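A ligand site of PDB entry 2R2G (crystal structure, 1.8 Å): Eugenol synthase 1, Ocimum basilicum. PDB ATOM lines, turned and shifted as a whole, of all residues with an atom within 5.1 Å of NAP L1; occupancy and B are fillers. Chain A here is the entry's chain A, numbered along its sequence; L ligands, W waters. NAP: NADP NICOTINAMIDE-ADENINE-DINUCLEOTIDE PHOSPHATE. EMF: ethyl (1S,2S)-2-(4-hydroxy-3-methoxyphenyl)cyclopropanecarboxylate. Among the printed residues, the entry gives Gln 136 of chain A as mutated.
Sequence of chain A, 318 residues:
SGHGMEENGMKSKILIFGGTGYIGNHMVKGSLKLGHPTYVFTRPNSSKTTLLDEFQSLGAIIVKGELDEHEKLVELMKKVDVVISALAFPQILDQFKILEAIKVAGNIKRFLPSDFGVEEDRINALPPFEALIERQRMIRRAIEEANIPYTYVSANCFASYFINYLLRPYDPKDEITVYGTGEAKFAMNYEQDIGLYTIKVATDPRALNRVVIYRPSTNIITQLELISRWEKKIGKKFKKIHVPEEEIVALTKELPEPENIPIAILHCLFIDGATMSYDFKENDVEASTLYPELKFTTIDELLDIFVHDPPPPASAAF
Water W1 lies within hydrogen-bond range of O2D of NAP L1 (2.6 Å), O of Asp 115 (2.7 Å) and NE2 of Gln 136 (2.8 Å).
Water W7 bridges an oxygen (O1A) of NAP L1 and the backbone NH (N) of Ala 317.
Water W5 lies within hydrogen-bond range of O2X of NAP L1, O of Phe 41, N of Thr 20 and N of Gly 18.
Water W11 lies within hydrogen-bond range of an oxygen (O1X) of NAP L1 (2.7 Å) and the side-chain amino group of Lys 48 (3.0 Å).
Water W2 lies within hydrogen-bond range of an oxygen (O2A) of NAP L1 and the side-chain amino group of Lys 48.
Water W3 lies within hydrogen-bond range of the side-chain amide oxygen (OE1) of Gln 91 (2.4 Å), the backbone NH (N) of Ala 88 (2.7 Å) and an oxygen (O4B) of NAP L1 (3.1 Å).
The side-chain amino group of Lys 48 sits at hydrogen-bond distance from the backbone carbonyl oxygen of Thr 20 (2.6 Å).
OG of Ser 46 sits at hydrogen-bond distance from N of Lys 48.
The backbone carbonyl oxygen (O) of Gly 117 sits at hydrogen-bond distance from the backbone NH (N) of Asn 156.
OG of Ser 114 lies within hydrogen-bond range of O of Leu 87 (2.6 Å).
The backbone carbonyl oxygen of Ser 114 sits at hydrogen-bond distance from the side-chain amide nitrogen of Gln 136 (3.0 Å).
Residues that only touch NAP L1: Phe 162 (3.1 Å), Phe 89 (3.2 Å), Ala 86 (3.3 Å), Asp 115 (3.5 Å), Ala 88 (3.7 Å), Gly 18 (3.7 Å), Gly 117 (3.8 Å) and Cys 157 (3.8 Å).
Hydrophobic or aromatic side chains that line NAP L1: Tyr 22, Ile 23, Leu 87, Ala 88, Phe 89, Phe 158 and Phe 162.
Of the 30 residues printed, 22 come within 4 Å of NAP L1.
The side-chain hydroxyl (OG1) of Thr 42 sits at hydrogen-bond distance from an oxygen (O2X) of NAP L1, 2.5 Å away.
An oxygen (O3B) of NAP L1 sits at hydrogen-bond distance from the side-chain hydroxyl (OG1) of Thr 20 (2.6 Å).
An oxygen (O2A) of NAP L1 lies within hydrogen-bond range of the backbone NH (N) of Tyr 22 (2.6 Å).
An oxygen (O1X) of NAP L1 lies within hydrogen-bond range of the side-chain hydroxyl of Ser 46, at 2.7 Å.
O of Asn 156 sits at hydrogen-bond distance from N7N of NAP L1 (2.7 Å).
An oxygen (O3D) of NAP L1 is in hydrogen-bond range of the backbone carbonyl oxygen of Ser 114 (3.5 Å).
O3D of NAP L1 lies within hydrogen-bond range of OG of Ser 114 (2.8 Å).
An oxygen (O3X) of NAP L1 is in hydrogen-bond range of the backbone NH (N) of Arg 43 (3.1 Å).
O3X of NAP L1 is in salt-bridge range of NE of Arg 43, 2.8 Å away.
N of Gly 21 is in hydrogen-bond range of O3B of NAP L1, at 3.0 Å.
An oxygen (O7N) of NAP L1 is in hydrogen-bond range of the backbone NH (N) of Phe 158.
An oxygen (O2N) of NAP L1 sits at hydrogen-bond distance from the backbone NH of Ile 23 (3.0 Å).
NZ of Lys 48 sits at hydrogen-bond distance from O3B of NAP L1 (3.1 Å).
A nitrogen (N7N) of NAP L1 lies within hydrogen-bond range of the backbone carbonyl oxygen (O) of Phe 116 (3.1 Å).
O of Leu 87 sits close to O3D of NAP L1 (3.4 Å).
NE2 of Gln 91 lies close to N6A of NAP L1 (3.3 Å).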
ATOM      1  N   GLY A  18       4.916  -3.571 -30.462  1.00  0.00           N
ATOM      2  CA  GLY A  18       4.534  -2.405 -29.682  1.00  0.00           C
ATOM      3  C   GLY A  18       5.054  -1.129 -30.322  1.00  0.00           C
ATOM      4  O   GLY A  18       5.175  -0.076 -29.677  1.00  0.00           O
ATOM      5  N   THR A  20       3.718   1.047 -32.112  1.00  0.00           N
ATOM      6  CA  THR A  20       2.805   2.188 -32.066  1.00  0.00           C
ATOM      7  C   THR A  20       2.735   2.777 -30.665  1.00  0.00           C
ATOM      8  O   THR A  20       2.039   3.773 -30.434  1.00  0.00           O
ATOM      9  CB  THR A  20       1.375   1.783 -32.486  1.00  0.00           C
ATOM     10  OG1 THR A  20       0.846   0.872 -31.519  1.00  0.00           O
ATOM     11  CG2 THR A  20       1.388   1.112 -33.854  1.00  0.00           C
ATOM     12  N   GLY A  21       3.455   2.161 -29.731  1.00  0.00           N
ATOM     13  CA  GLY A  21       3.436   2.599 -28.348  1.00  0.00           C
ATOM     14  C   GLY A  21       4.120   3.933 -28.057  1.00  0.00           C
ATOM     15  O   GLY A  21       4.711   4.542 -28.940  1.00  0.00           O
ATOM     16  N   TYR A  22       4.032   4.357 -26.802  1.00  0.00           N
ATOM     17  CA  TYR A  22       4.618   5.627 -26.391  1.00  0.00           C
ATOM     18  C   TYR A  22       6.101   5.698 -26.742  1.00  0.00           C
ATOM     19  O   TYR A  22       6.534   6.654 -27.381  1.00  0.00           O
ATOM     20  CB  TYR A  22       4.433   5.847 -24.876  1.00  0.00           C
ATOM     21  CG  TYR A  22       4.954   7.191 -24.439  1.00  0.00           C
ATOM     22  CD1 TYR A  22       4.277   8.362 -24.794  1.00  0.00           C
ATOM     23  CD2 TYR A  22       6.151   7.300 -23.738  1.00  0.00           C
ATOM     24  CE1 TYR A  22       4.789   9.620 -24.459  1.00  0.00           C
ATOM     25  CE2 TYR A  22       6.676   8.558 -23.410  1.00  0.00           C
ATOM     26  CZ  TYR A  22       5.992   9.707 -23.777  1.00  0.00           C
ATOM     27  OH  TYR A  22       6.508  10.955 -23.451  1.00  0.00           O
ATOM     28  N   ILE A  23       6.869   4.696 -26.330  1.00  0.00           N
ATOM     29  CA  ILE A  23       8.292   4.696 -26.640  1.00  0.00           C
ATOM     30  C   ILE A  23       8.562   3.924 -27.929  1.00  0.00           C
ATOM     31  O   ILE A  23       9.544   4.177 -28.622  1.00  0.00           O
ATOM     32  CB  ILE A  23       9.139   4.087 -25.483  1.00  0.00           C
ATOM     33  CG1 ILE A  23      10.624   4.424 -25.677  1.00  0.00           C
ATOM     34  CG2 ILE A  23       8.963   2.566 -25.433  1.00  0.00           C
ATOM     35  CD1 ILE A  23      10.936   5.918 -25.517  1.00  0.00           C
ATOM     36  N   GLY A  24       7.672   2.997 -28.262  1.00  0.00           N
ATOM     37  CA  GLY A  24       7.849   2.216 -29.471  1.00  0.00           C
ATOM     38  C   GLY A  24       7.890   3.019 -30.761  1.00  0.00           C
ATOM     39  O   GLY A  24       8.662   2.693 -31.671  1.00  0.00           O
ATOM     40  N   PHE A  41       4.742  -4.919 -35.937  1.00  0.00           N
ATOM     41  CA  PHE A  41       3.650  -5.842 -35.631  1.00  0.00           C
ATOM     42  C   PHE A  41       2.590  -5.050 -34.871  1.00  0.00           C
ATOM     43  O   PHE A  41       2.919  -4.349 -33.913  1.00  0.00           O
ATOM     44  CB  PHE A  41       4.157  -6.998 -34.770  1.00  0.00           C
ATOM     45  CG  PHE A  41       3.241  -8.196 -34.752  1.00  0.00           C
ATOM     46  CD1 PHE A  41       3.101  -8.995 -35.877  1.00  0.00           C
ATOM     47  CD2 PHE A  41       2.506  -8.505 -33.611  1.00  0.00           C
ATOM     48  CE1 PHE A  41       2.238 -10.103 -35.869  1.00  0.00           C
ATOM     49  CE2 PHE A  41       1.632  -9.596 -33.593  1.00  0.00           C
ATOM     50  CZ  PHE A  41       1.505 -10.395 -34.725  1.00  0.00           C
ATOM     51  N   THR A  42       1.349  -5.140 -35.296  1.00  0.00           N
ATOM     52  CA  THR A  42       0.283  -4.386 -34.637  1.00  0.00           C
ATOM     53  C   THR A  42      -1.041  -5.143 -34.679  1.00  0.00           C
ATOM     54  O   THR A  42      -1.306  -5.896 -35.621  1.00  0.00           O
ATOM     55  CB  THR A  42       0.123  -2.990 -35.308  1.00  0.00           C
ATOM     56  OG1 THR A  42      -0.942  -2.261 -34.676  1.00  0.00           O
ATOM     57  CG2 THR A  42      -0.185  -3.132 -36.788  1.00  0.00           C
ATOM     58  N   ARG A  43      -1.861  -4.978 -33.642  1.00  0.00           N
ATOM     59  CA  ARG A  43      -3.163  -5.649 -33.587  1.00  0.00           C
ATOM     60  C   ARG A  43      -4.090  -5.164 -34.691  1.00  0.00           C
ATOM     61  O   ARG A  43      -4.035  -4.013 -35.117  1.00  0.00           O
ATOM     62  CB  ARG A  43      -3.839  -5.395 -32.239  1.00  0.00           C
ATOM     63  CG  ARG A  43      -3.220  -6.111 -31.055  1.00  0.00           C
ATOM     64  CD  ARG A  43      -3.811  -5.590 -29.769  1.00  0.00           C
ATOM     65  NE  ARG A  43      -3.559  -4.158 -29.645  1.00  0.00           N
ATOM     66  CZ  ARG A  43      -4.190  -3.351 -28.805  1.00  0.00           C
ATOM     67  NH1 ARG A  43      -3.885  -2.058 -28.769  1.00  0.00           N
ATOM     68  NH2 ARG A  43      -5.141  -3.822 -28.014  1.00  0.00           N
ATOM     69  N   SER A  46      -6.213  -2.144 -33.526  1.00  0.00           N
ATOM     70  CA  SER A  46      -5.547  -0.969 -32.977  1.00  0.00           C
ATOM     71  C   SER A  46      -6.151   0.333 -33.484  1.00  0.00           C
ATOM     72  O   SER A  46      -6.628   0.406 -34.615  1.00  0.00           O
ATOM     73  CB  SER A  46      -4.057  -0.996 -33.310  1.00  0.00           C
ATOM     74  OG  SER A  46      -3.421   0.210 -32.907  1.00  0.00           O
ATOM     75  N   SER A  47      -6.141   1.356 -32.640  1.00  0.00           N
ATOM     76  CA  SER A  47      -6.674   2.657 -33.000  1.00  0.00           C
ATOM     77  C   SER A  47      -5.565   3.576 -33.485  1.00  0.00           C
ATOM     78  O   SER A  47      -5.786   4.761 -33.752  1.00  0.00           O
ATOM     79  CB  SER A  47      -7.376   3.290 -31.792  1.00  0.00           C
ATOM     80  OG  SER A  47      -6.452   3.514 -30.737  1.00  0.00           O
ATOM     81  N   LYS A  48      -4.357   3.028 -33.604  1.00  0.00           N
ATOM     82  CA  LYS A  48      -3.188   3.783 -34.045  1.00  0.00           C
ATOM     83  C   LYS A  48      -3.133   3.854 -35.577  1.00  0.00           C
ATOM     84  O   LYS A  48      -2.050   3.860 -36.160  1.00  0.00           O
ATOM     85  CB  LYS A  48      -1.910   3.122 -33.518  1.00  0.00           C
ATOM     86  CG  LYS A  48      -1.835   3.001 -31.997  1.00  0.00           C
ATOM     87  CD  LYS A  48      -1.679   4.359 -31.329  1.00  0.00           C
ATOM     88  CE  LYS A  48      -1.528   4.218 -29.815  1.00  0.00           C
ATOM     89  NZ  LYS A  48      -0.335   3.407 -29.443  1.00  0.00           N
ATOM     90  N   LEU A  67      -0.590 -11.732 -30.899  1.00  0.00           N
ATOM     91  CA  LEU A  67       0.546 -12.477 -30.366  1.00  0.00           C
ATOM     92  C   LEU A  67       0.217 -13.964 -30.274  1.00  0.00           C
ATOM     93  O   LEU A  67       1.113 -14.801 -30.258  1.00  0.00           O
ATOM     94  CB  LEU A  67       0.911 -11.959 -28.973  1.00  0.00           C
ATOM     95  CG  LEU A  67       1.457 -10.522 -28.914  1.00  0.00           C
ATOM     96  CD1 LEU A  67       1.717 -10.144 -27.457  1.00  0.00           C
ATOM     97  CD2 LEU A  67       2.733 -10.438 -29.725  1.00  0.00           C
ATOM     98  N   ALA A  86       8.586  -3.470 -27.261  1.00  0.00           N
ATOM     99  CA  ALA A  86       8.287  -2.268 -26.506  1.00  0.00           C
ATOM    100  C   ALA A  86       6.850  -2.373 -25.979  1.00  0.00           C
ATOM    101  O   ALA A  86       6.132  -1.382 -25.894  1.00  0.00           O
ATOM    102  CB  ALA A  86       8.421  -1.025 -27.401  1.00  0.00           C
ATOM    103  N   LEU A  87       6.439  -3.595 -25.633  1.00  0.00           N
ATOM    104  CA  LEU A  87       5.095  -3.836 -25.105  1.00  0.00           C
ATOM    105  C   LEU A  87       4.962  -3.257 -23.701  1.00  0.00           C
ATOM    106  O   LEU A  87       5.959  -3.070 -23.003  1.00  0.00           O
ATOM    107  CB  LEU A  87       4.798  -5.339 -25.071  1.00  0.00           C
ATOM    108  CG  LEU A  87       4.717  -6.041 -26.435  1.00  0.00           C
ATOM    109  CD1 LEU A  87       4.439  -7.530 -26.233  1.00  0.00           C
ATOM    110  CD2 LEU A  87       3.621  -5.391 -27.265  1.00  0.00           C
ATOM    111  N   ALA A  88       3.723  -2.993 -23.284  1.00  0.00           N
ATOM    112  CA  ALA A  88       3.439  -2.420 -21.968  1.00  0.00           C
ATOM    113  C   ALA A  88       3.417  -3.451 -20.828  1.00  0.00           C
ATOM    114  O   ALA A  88       3.373  -4.667 -21.068  1.00  0.00           O
ATOM    115  CB  ALA A  88       2.116  -1.664 -21.997  1.00  0.00           C
ATOM    116  N   PHE A  89       3.451  -2.948 -19.603  1.00  0.00           N
ATOM    117  CA  PHE A  89       3.457  -3.792 -18.406  1.00  0.00           C
ATOM    118  C   PHE A  89       2.440  -4.937 -18.382  1.00  0.00           C
ATOM    119  O   PHE A  89       2.790  -6.075 -18.072  1.00  0.00           O
ATOM    120  CB  PHE A  89       3.267  -2.941 -17.149  1.00  0.00           C
ATOM    121  CG  PHE A  89       4.582  -2.447 -16.559  1.00  0.00           C
ATOM    122  CD1 PHE A  89       4.787  -1.099 -16.309  1.00  0.00           C
ATOM    123  CD2 PHE A  89       5.578  -3.352 -16.220  1.00  0.00           C
ATOM    124  CE1 PHE A  89       5.964  -0.651 -15.733  1.00  0.00           C
ATOM    125  CE2 PHE A  89       6.765  -2.923 -15.641  1.00  0.00           C
ATOM    126  CZ  PHE A  89       6.968  -1.562 -15.395  1.00  0.00           C
ATOM    127  N   GLN A  91       1.403  -6.710 -20.555  1.00  0.00           N
ATOM    128  CA  GLN A  91       1.800  -7.780 -21.476  1.00  0.00           C
ATOM    129  C   GLN A  91       3.229  -8.290 -21.289  1.00  0.00           C
ATOM    130  O   GLN A  91       3.774  -8.914 -22.193  1.00  0.00           O
ATOM    131  CB  GLN A  91       1.616  -7.312 -22.917  1.00  0.00           C
ATOM    132  CG  GLN A  91       0.178  -7.350 -23.457  1.00  0.00           C
ATOM    133  CD  GLN A  91      -0.670  -6.155 -23.052  1.00  0.00           C
ATOM    134  OE1 GLN A  91      -0.319  -5.010 -23.329  1.00  0.00           O
ATOM    135  NE2 GLN A  91      -1.805  -6.421 -22.404  1.00  0.00           N
ATOM    136  N   SER A 114      11.142  -5.902 -23.426  1.00  0.00           N
ATOM    137  CA  SER A 114      10.594  -4.617 -23.005  1.00  0.00           C
ATOM    138  C   SER A 114      10.969  -4.210 -21.589  1.00  0.00           C
ATOM    139  O   SER A 114      10.272  -4.543 -20.631  1.00  0.00           O
ATOM    140  CB  SER A 114       9.066  -4.613 -23.146  1.00  0.00           C
ATOM    141  OG  SER A 114       8.560  -3.295 -22.962  1.00  0.00           O
ATOM    142  N   ASP A 115      12.081  -3.488 -21.477  1.00  0.00           N
ATOM    143  CA  ASP A 115      12.554  -2.985 -20.197  1.00  0.00           C
ATOM    144  C   ASP A 115      12.439  -1.465 -20.297  1.00  0.00           C
ATOM    145  O   ASP A 115      11.430  -0.883 -19.897  1.00  0.00           O
ATOM    146  CB  ASP A 115      14.021  -3.384 -19.960  1.00  0.00           C
ATOM    147  CG  ASP A 115      14.218  -4.882 -19.903  1.00  0.00           C
ATOM    148  OD1 ASP A 115      13.481  -5.560 -19.154  1.00  0.00           O
ATOM    149  OD2 ASP A 115      15.123  -5.388 -20.603  1.00  0.00           O
ATOM    150  N   PHE A 116      13.469  -0.848 -20.856  1.00  0.00           N
ATOM    151  CA  PHE A 116      13.519   0.597 -21.048  1.00  0.00           C
ATOM    152  C   PHE A 116      13.100   1.391 -19.812  1.00  0.00           C
ATOM    153  O   PHE A 116      12.266   2.289 -19.879  1.00  0.00           O
ATOM    154  CB  PHE A 116      12.655   0.973 -22.270  1.00  0.00           C
ATOM    155  CG  PHE A 116      12.966   0.148 -23.495  1.00  0.00           C
ATOM    156  CD1 PHE A 116      12.038  -0.753 -24.005  1.00  0.00           C
ATOM    157  CD2 PHE A 116      14.211   0.246 -24.111  1.00  0.00           C
ATOM    158  CE1 PHE A 116      12.342  -1.557 -25.111  1.00  0.00           C
ATOM    159  CE2 PHE A 116      14.532  -0.554 -25.216  1.00  0.00           C
ATOM    160  CZ  PHE A 116      13.593  -1.468 -25.715  1.00  0.00           C
ATOM    161  N   GLY A 117      13.708   1.059 -18.680  1.00  0.00           N
ATOM    162  CA  GLY A 117      13.402   1.738 -17.438  1.00  0.00           C
ATOM    163  C   GLY A 117      14.525   1.545 -16.444  1.00  0.00           C
ATOM    164  O   GLY A 117      15.686   1.852 -16.731  1.00  0.00           O
ATOM    165  N   GLN A 136       9.678  -9.034 -15.519  1.00  0.00           N
ATOM    166  CA  GLN A 136      10.691  -8.691 -16.519  1.00  0.00           C
ATOM    167  C   GLN A 136      11.946  -9.550 -16.282  1.00  0.00           C
ATOM    168  O   GLN A 136      12.636  -9.916 -17.239  1.00  0.00           O
ATOM    169  CB  GLN A 136      11.047  -7.184 -16.426  1.00  0.00           C
ATOM    170  CG  GLN A 136       9.853  -6.279 -16.731  1.00  0.00           C
ATOM    171  CD  GLN A 136      10.200  -4.810 -16.653  1.00  0.00           C
ATOM    172  OE1 GLN A 136      10.830  -4.360 -15.692  1.00  0.00           O
ATOM    173  NE2 GLN A 136       9.806  -4.048 -17.661  1.00  0.00           N
ATOM    174  N   ASN A 156      16.366   4.463 -18.176  1.00  0.00           N
ATOM    175  CA  ASN A 156      16.071   5.368 -17.073  1.00  0.00           C
ATOM    176  C   ASN A 156      14.776   6.141 -17.334  1.00  0.00           C
ATOM    177  O   ASN A 156      13.877   5.604 -17.971  1.00  0.00           O
ATOM    178  CB  ASN A 156      17.266   6.283 -16.814  1.00  0.00           C
ATOM    179  CG  ASN A 156      18.385   5.568 -16.089  1.00  0.00           C
ATOM    180  OD1 ASN A 156      18.138   4.755 -15.199  1.00  0.00           O
ATOM    181  ND2 ASN A 156      19.636   5.851 -16.462  1.00  0.00           N
ATOM    182  N   CYS A 157      14.647   7.391 -16.880  1.00  0.00           N
ATOM    183  CA  CYS A 157      13.373   8.113 -17.042  1.00  0.00           C
ATOM    184  C   CYS A 157      13.090   8.762 -18.403  1.00  0.00           C
ATOM    185  O   CYS A 157      13.927   9.479 -18.953  1.00  0.00           O
ATOM    186  CB  CYS A 157      13.240   9.185 -15.958  1.00  0.00           C
ATOM    187  SG  CYS A 157      13.320   8.553 -14.271  1.00  0.00           S
ATOM    188  N   PHE A 158      11.892   8.510 -18.936  1.00  0.00           N
ATOM    189  CA  PHE A 158      11.504   9.119 -20.209  1.00  0.00           C
ATOM    190  C   PHE A 158      11.311  10.597 -19.852  1.00  0.00           C
ATOM    191  O   PHE A 158      10.416  10.938 -19.066  1.00  0.00           O
ATOM    192  CB  PHE A 158      10.195   8.519 -20.739  1.00  0.00           C
ATOM    193  CG  PHE A 158      10.307   7.094 -21.263  1.00  0.00           C
ATOM    194  CD1 PHE A 158      11.509   6.396 -21.207  1.00  0.00           C
ATOM    195  CD2 PHE A 158       9.187   6.462 -21.783  1.00  0.00           C
ATOM    196  CE1 PHE A 158      11.573   5.058 -21.660  1.00  0.00           C
ATOM    197  CE2 PHE A 158       9.244   5.132 -22.234  1.00  0.00           C
ATOM    198  CZ  PHE A 158      10.441   4.427 -22.173  1.00  0.00           C
ATOM    199  N   TYR A 161       7.946  12.688 -20.677  1.00  0.00           N
ATOM    200  CA  TYR A 161       6.936  12.084 -19.827  1.00  0.00           C
ATOM    201  C   TYR A 161       7.032  12.647 -18.430  1.00  0.00           C
ATOM    202  O   TYR A 161       6.034  13.115 -17.871  1.00  0.00           O
ATOM    203  CB  TYR A 161       7.144  10.569 -19.780  1.00  0.00           C
ATOM    204  CG  TYR A 161       6.055   9.776 -19.068  1.00  0.00           C
ATOM    205  CD1 TYR A 161       5.064   9.120 -19.796  1.00  0.00           C
ATOM    206  CD2 TYR A 161       6.051   9.661 -17.679  1.00  0.00           C
ATOM    207  CE1 TYR A 161       4.087   8.354 -19.146  1.00  0.00           C
ATOM    208  CE2 TYR A 161       5.086   8.892 -17.023  1.00  0.00           C
ATOM    209  CZ  TYR A 161       4.113   8.242 -17.762  1.00  0.00           C
ATOM    210  OH  TYR A 161       3.163   7.463 -17.121  1.00  0.00           O
ATOM    211  N   PHE A 162       8.236  12.632 -17.860  1.00  0.00           N
ATOM    212  CA  PHE A 162       8.388  13.113 -16.505  1.00  0.00           C
ATOM    213  C   PHE A 162       8.480  14.600 -16.320  1.00  0.00           C
ATOM    214  O   PHE A 162       8.169  15.113 -15.232  1.00  0.00           O
ATOM    215  CB  PHE A 162       9.528  12.364 -15.799  1.00  0.00           C
ATOM    216  CG  PHE A 162       9.116  10.993 -15.358  1.00  0.00           C
ATOM    217  CD1 PHE A 162       9.376   9.873 -16.143  1.00  0.00           C
ATOM    218  CD2 PHE A 162       8.365  10.830 -14.192  1.00  0.00           C
ATOM    219  CE1 PHE A 162       8.881   8.617 -15.785  1.00  0.00           C
ATOM    220  CE2 PHE A 162       7.870   9.571 -13.820  1.00  0.00           C
ATOM    221  CZ  PHE A 162       8.126   8.477 -14.615  1.00  0.00           C
ATOM    222  N   ALA A 316       1.316   6.010 -18.769  1.00  0.00           N
ATOM    223  CA  ALA A 316       1.563   4.593 -19.011  1.00  0.00           C
ATOM    224  C   ALA A 316       0.340   3.757 -18.638  1.00  0.00           C
ATOM    225  O   ALA A 316      -0.467   4.158 -17.795  1.00  0.00           O
ATOM    226  CB  ALA A 316       2.778   4.126 -18.222  1.00  0.00           C
ATOM    227  N   ALA A 317       0.212   2.591 -19.276  1.00  0.00           N
ATOM    228  CA  ALA A 317      -0.905   1.692 -19.018  1.00  0.00           C
ATOM    229  C   ALA A 317      -0.526   0.694 -17.939  1.00  0.00           C
ATOM    230  O   ALA A 317       0.589   0.176 -17.934  1.00  0.00           O
ATOM    231  CB  ALA A 317      -1.296   0.966 -20.299  1.00  0.00           C
HETATM  232  PA  NAP L   1       2.179   1.618 -24.606  1.00  0.00           P
HETATM  233  O1A NAP L   1       1.217   1.631 -23.481  1.00  0.00           O
HETATM  234  O2A NAP L   1       2.367   2.811 -25.457  1.00  0.00           O
HETATM  235  O5B NAP L   1       1.819   0.313 -25.446  1.00  0.00           O
HETATM  236  C5B NAP L   1       2.735  -0.189 -26.425  1.00  0.00           C
HETATM  237  C4B NAP L   1       1.927  -0.950 -27.437  1.00  0.00           C
HETATM  238  O4B NAP L   1       1.246  -2.229 -26.991  1.00  0.00           O
HETATM  239  C3B NAP L   1       0.655  -0.307 -27.995  1.00  0.00           C
HETATM  240  O3B NAP L   1       1.015   0.710 -28.907  1.00  0.00           O
HETATM  241  C2B NAP L   1      -0.152  -1.442 -28.659  1.00  0.00           C
HETATM  242  O2B NAP L   1       0.128  -1.545 -30.047  1.00  0.00           O
HETATM  243  C1B NAP L   1       0.277  -2.686 -27.911  1.00  0.00           C
HETATM  244  N9A NAP L   1      -0.774  -3.327 -27.120  1.00  0.00           N
HETATM  245  C8A NAP L   1      -1.652  -2.710 -26.240  1.00  0.00           C
HETATM  246  N7A NAP L   1      -2.492  -3.538 -25.661  1.00  0.00           N
HETATM  247  C5A NAP L   1      -2.158  -4.747 -26.185  1.00  0.00           C
HETATM  248  C6A NAP L   1      -2.689  -6.055 -25.968  1.00  0.00           C
HETATM  249  N6A NAP L   1      -3.710  -6.265 -25.125  1.00  0.00           N
HETATM  250  N1A NAP L   1      -2.123  -7.088 -26.665  1.00  0.00           N
HETATM  251  C2A NAP L   1      -1.085  -6.871 -27.521  1.00  0.00           C
HETATM  252  N3A NAP L   1      -0.508  -5.670 -27.799  1.00  0.00           N
HETATM  253  C4A NAP L   1      -1.101  -4.653 -27.091  1.00  0.00           C
HETATM  254  O3  NAP L   1       3.607   1.140 -23.989  1.00  0.00           O
HETATM  255  PN  NAP L   1       4.672   2.187 -23.438  1.00  0.00           P
HETATM  256  O1N NAP L   1       3.996   3.214 -22.603  1.00  0.00           O
HETATM  257  O2N NAP L   1       5.407   2.669 -24.647  1.00  0.00           O
HETATM  258  O5D NAP L   1       5.699   1.322 -22.579  1.00  0.00           O
HETATM  259  C5D NAP L   1       6.597   0.360 -23.183  1.00  0.00           C
HETATM  260  C4D NAP L   1       7.696   0.009 -22.212  1.00  0.00           C
HETATM  261  O4D NAP L   1       8.308   1.255 -21.753  1.00  0.00           O
HETATM  262  C3D NAP L   1       7.212  -0.797 -20.986  1.00  0.00           C
HETATM  263  O3D NAP L   1       8.113  -1.836 -20.655  1.00  0.00           O
HETATM  264  C2D NAP L   1       7.087   0.292 -19.964  1.00  0.00           C
HETATM  265  O2D NAP L   1       7.176  -0.235 -18.653  1.00  0.00           O
HETATM  266  C1D NAP L   1       8.186   1.258 -20.319  1.00  0.00           C
HETATM  267  N1N NAP L   1       7.918   2.626 -19.769  1.00  0.00           N
HETATM  268  C2N NAP L   1       8.992   3.270 -19.156  1.00  0.00           C
HETATM  269  C3N NAP L   1       8.922   4.635 -18.849  1.00  0.00           C
HETATM  270  C7N NAP L   1      10.108   5.378 -18.270  1.00  0.00           C
HETATM  271  O7N NAP L   1       9.960   6.515 -17.801  1.00  0.00           O
HETATM  272  N7N NAP L   1      11.306   4.764 -18.314  1.00  0.00           N
HETATM  273  C4N NAP L   1       7.696   5.336 -19.114  1.00  0.00           C
HETATM  274  C5N NAP L   1       6.610   4.665 -19.734  1.00  0.00           C
HETATM  275  C6N NAP L   1       6.733   3.317 -20.077  1.00  0.00           C
HETATM  276  P2B NAP L   1      -0.980  -1.841 -31.188  1.00  0.00           P
HETATM  277  O1X NAP L   1      -2.195  -0.996 -30.886  1.00  0.00           O
HETATM  278  O2X NAP L   1      -0.211  -1.482 -32.433  1.00  0.00           O
HETATM  279  O3X NAP L   1      -1.294  -3.339 -31.111  1.00  0.00           O
HETATM  280  O9  EMF L   2       3.931   4.923 -13.294  1.00  0.00           O
HETATM  281  C9  EMF L   2       4.875   5.299 -13.988  1.00  0.00           C
HETATM  282  O10 EMF L   2       5.172   6.730 -14.049  1.00  0.00           O
HETATM  283  C11 EMF L   2       4.709   7.625 -13.034  1.00  0.00           C
HETATM  284  C12 EMF L   2       5.371   7.297 -11.711  1.00  0.00           C
HETATM  285  C8  EMF L   2       5.687   4.309 -14.767  1.00  0.00           C
HETATM  286  C14 EMF L   2       5.715   4.498 -16.278  1.00  0.00           C
HETATM  287  C7  EMF L   2       6.962   4.855 -15.450  1.00  0.00           C
HETATM  288  C1  EMF L   2       8.080   3.825 -15.402  1.00  0.00           C
HETATM  289  C2  EMF L   2       9.387   4.229 -14.988  1.00  0.00           C
HETATM  290  C3  EMF L   2      10.446   3.282 -14.935  1.00  0.00           C
HETATM  291  O3  EMF L   2      11.710   3.641 -14.537  1.00  0.00           O
HETATM  292  C13 EMF L   2      12.468   4.608 -15.260  1.00  0.00           C
HETATM  293  C6  EMF L   2       7.842   2.456 -15.773  1.00  0.00           C
HETATM  294  C5  EMF L   2       8.866   1.488 -15.740  1.00  0.00           C
HETATM  295  C4  EMF L   2      10.171   1.845 -15.327  1.00  0.00           C
HETATM  296  O4  EMF L   2      11.171   0.924 -15.279  1.00  0.00           O
HETATM  297  O   HOH W   1       9.466  -1.250 -18.082  1.00  0.00           O
HETATM  298  O   HOH W   2       0.220   4.198 -26.616  1.00  0.00           O
HETATM  299  O   HOH W   3       1.567  -4.121 -24.533  1.00  0.00           O
HETATM  300  O   HOH W   4       5.868   1.405 -26.831  1.00  0.00           O
HETATM  301  O   HOH W   5       2.421  -1.918 -32.235  1.00  0.00           O
HETATM  302  O   HOH W   6      -1.019  -0.214 -23.743  1.00  0.00           O
HETATM  303  O   HOH W   7       2.012   2.007 -21.058  1.00  0.00           O
HETATM  304  O   HOH W   8      -1.926  -9.260 -29.633  1.00  0.00           O
HETATM  305  O   HOH W   9       0.465  -5.404 -30.678  1.00  0.00           O
HETATM  306  O   HOH W  10       3.685   5.800 -21.644  1.00  0.00           O
HETATM  307  O   HOH W  11      -2.316   1.178 -29.318  1.00  0.00           O
